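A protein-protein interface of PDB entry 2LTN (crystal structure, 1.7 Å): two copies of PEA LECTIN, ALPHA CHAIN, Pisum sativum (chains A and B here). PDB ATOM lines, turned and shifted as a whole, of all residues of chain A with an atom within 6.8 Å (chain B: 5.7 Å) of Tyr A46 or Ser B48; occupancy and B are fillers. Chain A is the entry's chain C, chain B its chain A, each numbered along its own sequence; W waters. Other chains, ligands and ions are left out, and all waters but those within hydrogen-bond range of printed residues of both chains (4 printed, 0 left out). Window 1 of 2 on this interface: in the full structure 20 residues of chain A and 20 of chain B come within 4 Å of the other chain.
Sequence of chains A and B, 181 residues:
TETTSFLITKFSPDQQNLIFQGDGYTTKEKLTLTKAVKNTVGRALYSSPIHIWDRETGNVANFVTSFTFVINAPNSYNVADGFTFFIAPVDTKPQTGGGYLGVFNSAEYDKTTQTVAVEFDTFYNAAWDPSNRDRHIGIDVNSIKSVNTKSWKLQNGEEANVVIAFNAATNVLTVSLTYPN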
ATOM      1  N   THR A   4      -8.875 -25.221  -2.810  1.00  0.00           N
ATOM      2  CA  THR A   4      -8.719 -24.344  -1.620  1.00  0.00           C
ATOM      3  C   THR A   4      -7.647 -23.350  -1.995  1.00  0.00           C
ATOM      4  O   THR A   4      -6.605 -23.797  -2.535  1.00  0.00           O
ATOM      5  CB  THR A   4      -8.399 -25.076  -0.288  1.00  0.00           C
ATOM      6  OG1 THR A   4      -9.474 -25.972   0.055  1.00  0.00           O
ATOM      7  CG2 THR A   4      -8.061 -24.149   0.881  1.00  0.00           C
ATOM      8  N   SER A   5      -7.889 -22.025  -1.851  1.00  0.00           N
ATOM      9  CA  SER A   5      -6.817 -21.067  -2.223  1.00  0.00           C
ATOM     10  C   SER A   5      -6.836 -19.914  -1.225  1.00  0.00           C
ATOM     11  O   SER A   5      -7.907 -19.646  -0.656  1.00  0.00           O
ATOM     12  CB  SER A   5      -6.877 -20.524  -3.654  1.00  0.00           C
ATOM     13  OG  SER A   5      -7.313 -21.527  -4.578  1.00  0.00           O
ATOM     14  N   PHE A   6      -5.698 -19.323  -0.950  1.00  0.00           N
ATOM     15  CA  PHE A   6      -5.648 -18.108  -0.103  1.00  0.00           C
ATOM     16  C   PHE A   6      -4.400 -17.359  -0.501  1.00  0.00           C
ATOM     17  O   PHE A   6      -3.432 -17.951  -1.047  1.00  0.00           O
ATOM     18  CB  PHE A   6      -5.832 -18.338   1.378  1.00  0.00           C
ATOM     19  CG  PHE A   6      -4.698 -19.115   2.026  1.00  0.00           C
ATOM     20  CD1 PHE A   6      -4.865 -20.470   2.261  1.00  0.00           C
ATOM     21  CD2 PHE A   6      -3.543 -18.431   2.378  1.00  0.00           C
ATOM     22  CE1 PHE A   6      -3.781 -21.203   2.825  1.00  0.00           C
ATOM     23  CE2 PHE A   6      -2.440 -19.165   2.932  1.00  0.00           C
ATOM     24  CZ  PHE A   6      -2.644 -20.509   3.177  1.00  0.00           C
ATOM     25  N   ILE A   8      -2.147 -14.012   1.389  1.00  0.00           N
ATOM     26  CA  ILE A   8      -2.005 -13.037   2.452  1.00  0.00           C
ATOM     27  C   ILE A   8      -0.699 -12.284   2.198  1.00  0.00           C
ATOM     28  O   ILE A   8       0.346 -12.960   2.331  1.00  0.00           O
ATOM     29  CB  ILE A   8      -2.022 -13.662   3.868  1.00  0.00           C
ATOM     30  CG1 ILE A   8      -3.277 -14.573   4.094  1.00  0.00           C
ATOM     31  CG2 ILE A   8      -1.969 -12.619   5.019  1.00  0.00           C
ATOM     32  CD1 ILE A   8      -3.127 -15.463   5.359  1.00  0.00           C
ATOM     33  N   GLN A  16      -7.401 -14.001  12.296  1.00  0.00           N
ATOM     34  CA  GLN A  16      -8.284 -15.057  12.723  1.00  0.00           C
ATOM     35  C   GLN A  16      -8.340 -16.250  11.812  1.00  0.00           C
ATOM     36  O   GLN A  16      -8.924 -17.251  12.314  1.00  0.00           O
ATOM     37  CB  GLN A  16      -9.722 -14.487  13.051  1.00  0.00           C
ATOM     38  CG  GLN A  16      -9.639 -13.426  14.114  1.00  0.00           C
ATOM     39  CD  GLN A  16     -11.022 -12.945  14.636  1.00  0.00           C
ATOM     40  OE1 GLN A  16     -11.970 -13.619  14.273  1.00  0.00           O
ATOM     41  NE2 GLN A  16     -10.978 -11.870  15.403  1.00  0.00           N
ATOM     42  N   ASN A  17      -7.783 -16.186  10.615  1.00  0.00           N
ATOM     43  CA  ASN A  17      -7.815 -17.360   9.742  1.00  0.00           C
ATOM     44  C   ASN A  17      -6.499 -18.206   9.963  1.00  0.00           C
ATOM     45  O   ASN A  17      -6.375 -19.074   9.112  1.00  0.00           O
ATOM     46  CB  ASN A  17      -8.017 -17.144   8.277  1.00  0.00           C
ATOM     47  CG  ASN A  17      -7.132 -16.105   7.697  1.00  0.00           C
ATOM     48  OD1 ASN A  17      -6.314 -15.438   8.338  1.00  0.00           O
ATOM     49  ND2 ASN A  17      -7.222 -15.934   6.385  1.00  0.00           N
ATOM     50  N   LEU A  18      -5.769 -17.794  10.931  1.00  0.00           N
ATOM     51  CA  LEU A  18      -4.547 -18.717  11.239  1.00  0.00           C
ATOM     52  C   LEU A  18      -4.688 -19.169  12.670  1.00  0.00           C
ATOM     53  O   LEU A  18      -5.367 -18.562  13.530  1.00  0.00           O
ATOM     54  CB  LEU A  18      -3.292 -17.853  11.063  1.00  0.00           C
ATOM     55  CG  LEU A  18      -2.562 -17.866   9.733  1.00  0.00           C
ATOM     56  CD1 LEU A  18      -3.426 -17.817   8.525  1.00  0.00           C
ATOM     57  CD2 LEU A  18      -1.578 -16.643   9.773  1.00  0.00           C
ATOM     58  N   ILE A  19      -4.058 -20.358  12.948  1.00  0.00           N
ATOM     59  CA  ILE A  19      -4.039 -20.891  14.331  1.00  0.00           C
ATOM     60  C   ILE A  19      -2.566 -20.729  14.818  1.00  0.00           C
ATOM     61  O   ILE A  19      -1.714 -21.194  14.029  1.00  0.00           O
ATOM     62  CB  ILE A  19      -4.496 -22.378  14.338  1.00  0.00           C
ATOM     63  CG1 ILE A  19      -6.006 -22.535  13.920  1.00  0.00           C
ATOM     64  CG2 ILE A  19      -4.189 -23.046  15.713  1.00  0.00           C
ATOM     65  CD1 ILE A  19      -6.346 -24.034  13.587  1.00  0.00           C
ATOM     66  N   ALA A  44       2.397 -21.715  13.053  1.00  0.00           N
ATOM     67  CA  ALA A  44       1.150 -21.013  12.567  1.00  0.00           C
ATOM     68  C   ALA A  44       0.575 -21.925  11.477  1.00  0.00           C
ATOM     69  O   ALA A  44       1.323 -22.417  10.606  1.00  0.00           O
ATOM     70  CB  ALA A  44       1.491 -19.664  12.015  1.00  0.00           C
ATOM     71  N   LEU A  45      -0.754 -22.192  11.540  1.00  0.00           N
ATOM     72  CA  LEU A  45      -1.400 -23.076  10.610  1.00  0.00           C
ATOM     73  C   LEU A  45      -2.650 -22.329   9.922  1.00  0.00           C
ATOM     74  O   LEU A  45      -3.150 -21.512  10.707  1.00  0.00           O
ATOM     75  CB  LEU A  45      -2.011 -24.261  11.382  1.00  0.00           C
ATOM     76  CG  LEU A  45      -0.867 -25.103  12.116  1.00  0.00           C
ATOM     77  CD1 LEU A  45      -1.488 -25.265  13.490  1.00  0.00           C
ATOM     78  CD2 LEU A  45      -0.876 -26.419  11.407  1.00  0.00           C
ATOM     79  N   TYR A  46      -2.784 -22.759   8.697  1.00  0.00           N
ATOM     80  CA  TYR A  46      -4.066 -22.111   8.084  1.00  0.00           C
ATOM     81  C   TYR A  46      -5.191 -22.821   8.791  1.00  0.00           C
ATOM     82  O   TYR A  46      -5.248 -24.035   9.056  1.00  0.00           O
ATOM     83  CB  TYR A  46      -4.034 -22.427   6.620  1.00  0.00           C
ATOM     84  CG  TYR A  46      -5.269 -21.761   5.981  1.00  0.00           C
ATOM     85  CD1 TYR A  46      -6.171 -22.534   5.291  1.00  0.00           C
ATOM     86  CD2 TYR A  46      -5.328 -20.361   6.027  1.00  0.00           C
ATOM     87  CE1 TYR A  46      -7.224 -21.872   4.619  1.00  0.00           C
ATOM     88  CE2 TYR A  46      -6.425 -19.722   5.372  1.00  0.00           C
ATOM     89  CZ  TYR A  46      -7.320 -20.514   4.694  1.00  0.00           C
ATOM     90  OH  TYR A  46      -8.356 -19.823   4.025  1.00  0.00           O
ATOM     91  N   SER A  47      -6.274 -21.944   9.093  1.00  0.00           N
ATOM     92  CA  SER A  47      -7.423 -22.454   9.792  1.00  0.00           C
ATOM     93  C   SER A  47      -8.137 -23.628   9.175  1.00  0.00           C
ATOM     94  O   SER A  47      -8.541 -24.557   9.957  1.00  0.00           O
ATOM     95  CB  SER A  47      -8.388 -21.195   9.976  1.00  0.00           C
ATOM     96  OG  SER A  47      -9.571 -21.634  10.576  1.00  0.00           O
ATOM     97  N   SER A  48      -8.393 -23.650   7.889  1.00  0.00           N
ATOM     98  CA  SER A  48      -9.201 -24.704   7.284  1.00  0.00           C
ATOM     99  C   SER A  48      -8.398 -25.989   6.988  1.00  0.00           C
ATOM    100  O   SER A  48      -7.362 -25.802   6.384  1.00  0.00           O
ATOM    101  CB  SER A  48      -9.792 -24.177   5.958  1.00  0.00           C
ATOM    102  OG  SER A  48     -10.607 -25.175   5.345  1.00  0.00           O
ATOM    103  N   PRO A  49      -9.024 -27.098   7.289  1.00  0.00           N
ATOM    104  CA  PRO A  49      -8.436 -28.396   6.866  1.00  0.00           C
ATOM    105  C   PRO A  49      -8.396 -28.366   5.368  1.00  0.00           C
ATOM    106  O   PRO A  49      -9.292 -27.725   4.711  1.00  0.00           O
ATOM    107  CB  PRO A  49      -9.487 -29.419   7.341  1.00  0.00           C
ATOM    108  CG  PRO A  49     -10.063 -28.741   8.577  1.00  0.00           C
ATOM    109  CD  PRO A  49     -10.215 -27.280   8.080  1.00  0.00           C
ATOM    110  N   ILE A  50      -7.481 -29.026   4.708  1.00  0.00           N
ATOM    111  CA  ILE A  50      -7.270 -29.124   3.297  1.00  0.00           C
ATOM    112  C   ILE A  50      -7.431 -30.585   2.851  1.00  0.00           C
ATOM    113  O   ILE A  50      -6.920 -31.471   3.563  1.00  0.00           O
ATOM    114  CB  ILE A  50      -5.814 -28.698   2.871  1.00  0.00           C
ATOM    115  CG1 ILE A  50      -5.448 -27.331   3.532  1.00  0.00           C
ATOM    116  CG2 ILE A  50      -5.646 -28.604   1.350  1.00  0.00           C
ATOM    117  CD1 ILE A  50      -6.331 -26.226   2.942  1.00  0.00           C
ATOM    118  N   THR B   4      -9.392 -15.267  -0.314  1.00  0.00           N
ATOM    119  CA  THR B   4      -9.822 -16.574   0.159  1.00  0.00           C
ATOM    120  C   THR B   4     -10.682 -17.151  -0.999  1.00  0.00           C
ATOM    121  O   THR B   4     -11.586 -16.339  -1.360  1.00  0.00           O
ATOM    122  CB  THR B   4     -10.662 -16.594   1.443  1.00  0.00           C
ATOM    123  OG1 THR B   4      -9.851 -16.010   2.533  1.00  0.00           O
ATOM    124  CG2 THR B   4     -11.279 -17.916   1.888  1.00  0.00           C
ATOM    125  N   ASN B  17     -13.832 -29.320   6.010  1.00  0.00           N
ATOM    126  CA  ASN B  17     -13.679 -27.898   5.839  1.00  0.00           C
ATOM    127  C   ASN B  17     -15.087 -27.175   6.025  1.00  0.00           C
ATOM    128  O   ASN B  17     -14.981 -25.972   5.788  1.00  0.00           O
ATOM    129  CB  ASN B  17     -13.011 -27.468   4.581  1.00  0.00           C
ATOM    130  CG  ASN B  17     -13.632 -27.898   3.275  1.00  0.00           C
ATOM    131  OD1 ASN B  17     -14.579 -28.703   3.298  1.00  0.00           O
ATOM    132  ND2 ASN B  17     -13.091 -27.469   2.133  1.00  0.00           N
ATOM    133  N   TYR B  46     -18.570 -22.297   6.097  1.00  0.00           N
ATOM    134  CA  TYR B  46     -17.120 -22.577   5.636  1.00  0.00           C
ATOM    135  C   TYR B  46     -16.287 -22.419   6.918  1.00  0.00           C
ATOM    136  O   TYR B  46     -16.421 -21.574   7.768  1.00  0.00           O
ATOM    137  CB  TYR B  46     -16.633 -21.656   4.532  1.00  0.00           C
ATOM    138  CG  TYR B  46     -15.241 -21.997   4.005  1.00  0.00           C
ATOM    139  CD1 TYR B  46     -14.244 -21.077   4.035  1.00  0.00           C
ATOM    140  CD2 TYR B  46     -15.033 -23.281   3.489  1.00  0.00           C
ATOM    141  CE1 TYR B  46     -12.945 -21.396   3.544  1.00  0.00           C
ATOM    142  CE2 TYR B  46     -13.707 -23.587   2.964  1.00  0.00           C
ATOM    143  CZ  TYR B  46     -12.744 -22.637   3.011  1.00  0.00           C
ATOM    144  OH  TYR B  46     -11.521 -23.021   2.525  1.00  0.00           O
ATOM    145  N   SER B  47     -15.288 -23.415   7.028  1.00  0.00           N
ATOM    146  CA  SER B  47     -14.446 -23.441   8.260  1.00  0.00           C
ATOM    147  C   SER B  47     -13.642 -22.177   8.528  1.00  0.00           C
ATOM    148  O   SER B  47     -13.517 -21.751   9.717  1.00  0.00           O
ATOM    149  CB  SER B  47     -13.474 -24.680   8.085  1.00  0.00           C
ATOM    150  OG  SER B  47     -12.570 -24.630   9.170  1.00  0.00           O
ATOM    151  N   SER B  48     -13.056 -21.647   7.468  1.00  0.00           N
ATOM    152  CA  SER B  48     -12.162 -20.454   7.719  1.00  0.00           C
ATOM    153  C   SER B  48     -12.923 -19.140   7.893  1.00  0.00           C
ATOM    154  O   SER B  48     -13.751 -18.864   7.010  1.00  0.00           O
ATOM    155  CB  SER B  48     -11.086 -20.351   6.679  1.00  0.00           C
ATOM    156  OG  SER B  48     -10.201 -19.277   7.033  1.00  0.00           O
ATOM    157  N   PRO B  49     -12.540 -18.387   8.876  1.00  0.00           N
ATOM    158  CA  PRO B  49     -13.053 -16.988   9.008  1.00  0.00           C
ATOM    159  C   PRO B  49     -12.541 -16.271   7.798  1.00  0.00           C
ATOM    160  O   PRO B  49     -11.471 -16.586   7.191  1.00  0.00           O
ATOM    161  CB  PRO B  49     -12.344 -16.468  10.287  1.00  0.00           C
ATOM    162  CG  PRO B  49     -12.091 -17.775  11.053  1.00  0.00           C
ATOM    163  CD  PRO B  49     -11.584 -18.699   9.956  1.00  0.00           C
ATOM    164  N   ILE B  50     -13.318 -15.313   7.276  1.00  0.00           N
ATOM    165  CA  ILE B  50     -13.020 -14.505   6.093  1.00  0.00           C
ATOM    166  C   ILE B  50     -12.789 -13.031   6.503  1.00  0.00           C
ATOM    167  O   ILE B  50     -13.613 -12.560   7.335  1.00  0.00           O
ATOM    168  CB  ILE B  50     -14.230 -14.586   5.078  1.00  0.00           C
ATOM    169  CG1 ILE B  50     -14.593 -16.044   4.581  1.00  0.00           C
ATOM    170  CG2 ILE B  50     -13.979 -13.651   3.885  1.00  0.00           C
ATOM    171  CD1 ILE B  50     -13.367 -16.776   4.066  1.00  0.00           C
HETATM  172  O   HOH W   1      -9.579 -20.999   1.774  1.00  0.00           O
HETATM  173  O   HOH W   2     -10.596 -25.872   2.637  1.00  0.00           O
HETATM  174  O   HOH W   3      -9.435 -17.142   5.036  1.00  0.00           O
HETATM  175  O   HOH W   4     -11.503 -23.389  11.422  1.00  0.00           O
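Water W4 lies within hydrogen-bond range of OG of Ser A47 (2.7 Å) and OG of Ser B47 (2.8 Å).
Water W3 lies within hydrogen-bond range of the side-chain hydroxyl (OG1) of Thr B4 (2.8 Å), the side-chain amide nitrogen (ND2) of Asn A17 (2.9 Å), the backbone carbonyl oxygen (O) of Pro B49 (3.0 Å), the side-chain hydroxyl (OG) of Ser B48 (3.0 Å) and the side-chain hydroxyl (OH) of Tyr A46 (3.1 Å).
Water W2 lies within hydrogen-bond range of the side-chain hydroxyl of Ser A48 (2.8 Å), the side-chain hydroxyl of Thr A4 (2.8 Å), the side-chain hydroxyl of Tyr B46 (3.0 Å), the side-chain amide nitrogen of Asn B17 (3.0 Å) and the backbone carbonyl oxygen of Pro A49 (3.1 Å).
Water W1 lies within hydrogen-bond range of the side-chain hydroxyl of Tyr A46, the side-chain hydroxyl of Tyr B46 and the backbone carbonyl oxygen of Ser A5.
The backbone NH (N) of Ser B47 lies within hydrogen-bond range of the backbone carbonyl oxygen (O) of Asn B17 (2.9 Å).
O of Asn A17 is in hydrogen-bond range of N of Ser A47, 2.9 Å away.
Thr A4 touches Tyr B46, but with the chains exchanged Tyr A46 does not touch Thr B4 (4.1 Å).
Asn A17 touches Pro B49, and with the chains exchanged Pro A49 touches Asn B17.
Ser A47 touches Ser B48, and with the chains exchanged Ser A48 touches Ser B47.
Ser A47 touches Pro B49, and with the chains exchanged Pro A49 touches Ser B47.
7 positions are printed for both chains.
Of the 15 printed residues of chain A, 8 touch a printed residue of chain B.
Of the 7 printed residues of chain B, 6 touch a printed residue of chain A.
Along chain B the printed residues that touch a printed residue of chain A span positions 4 to 49.
Tyr A46 touches just one residue of chain B: Ser B48.
Printed residues of chain B within 4 Å of Pro A49: Asn B17 and Ser B47.
Ile A50 touches none of the printed residues of chain B.
Of the printed residues of chain A, Tyr B46 touches Thr A4 (3.99 Å) and Ser A48 (3.7 Å).
Ser B48 touches three residues of chain A.
Ile B50 touches none of the printed residues of chain A.
The nearest residue of chain A that does not touch Ser B48 is Ser A48 (4.1 Å).
Thr B4 touches Ser A5 (CA to O, 3.7 Å).
CG of Pro B49 touches O of Gln A16, 3.4 Å away.
CB of Asn A17 touches OG of Ser B48, at 3.3 Å.
CB of Asn A17 touches O of Pro B49, at 3.7 Å.
Ser B48 touches Tyr A46.
CB of Ser A47 touches OG of Ser B48 (3.95 Å).
Ser A47 touches Pro B49 (OG to CD, 3.6 Å).
Asn B17 touches Ser A48.
Ser A48 touches Tyr B46 (OG to OH, 3.7 Å).
Pro A49 touches Asn B17.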
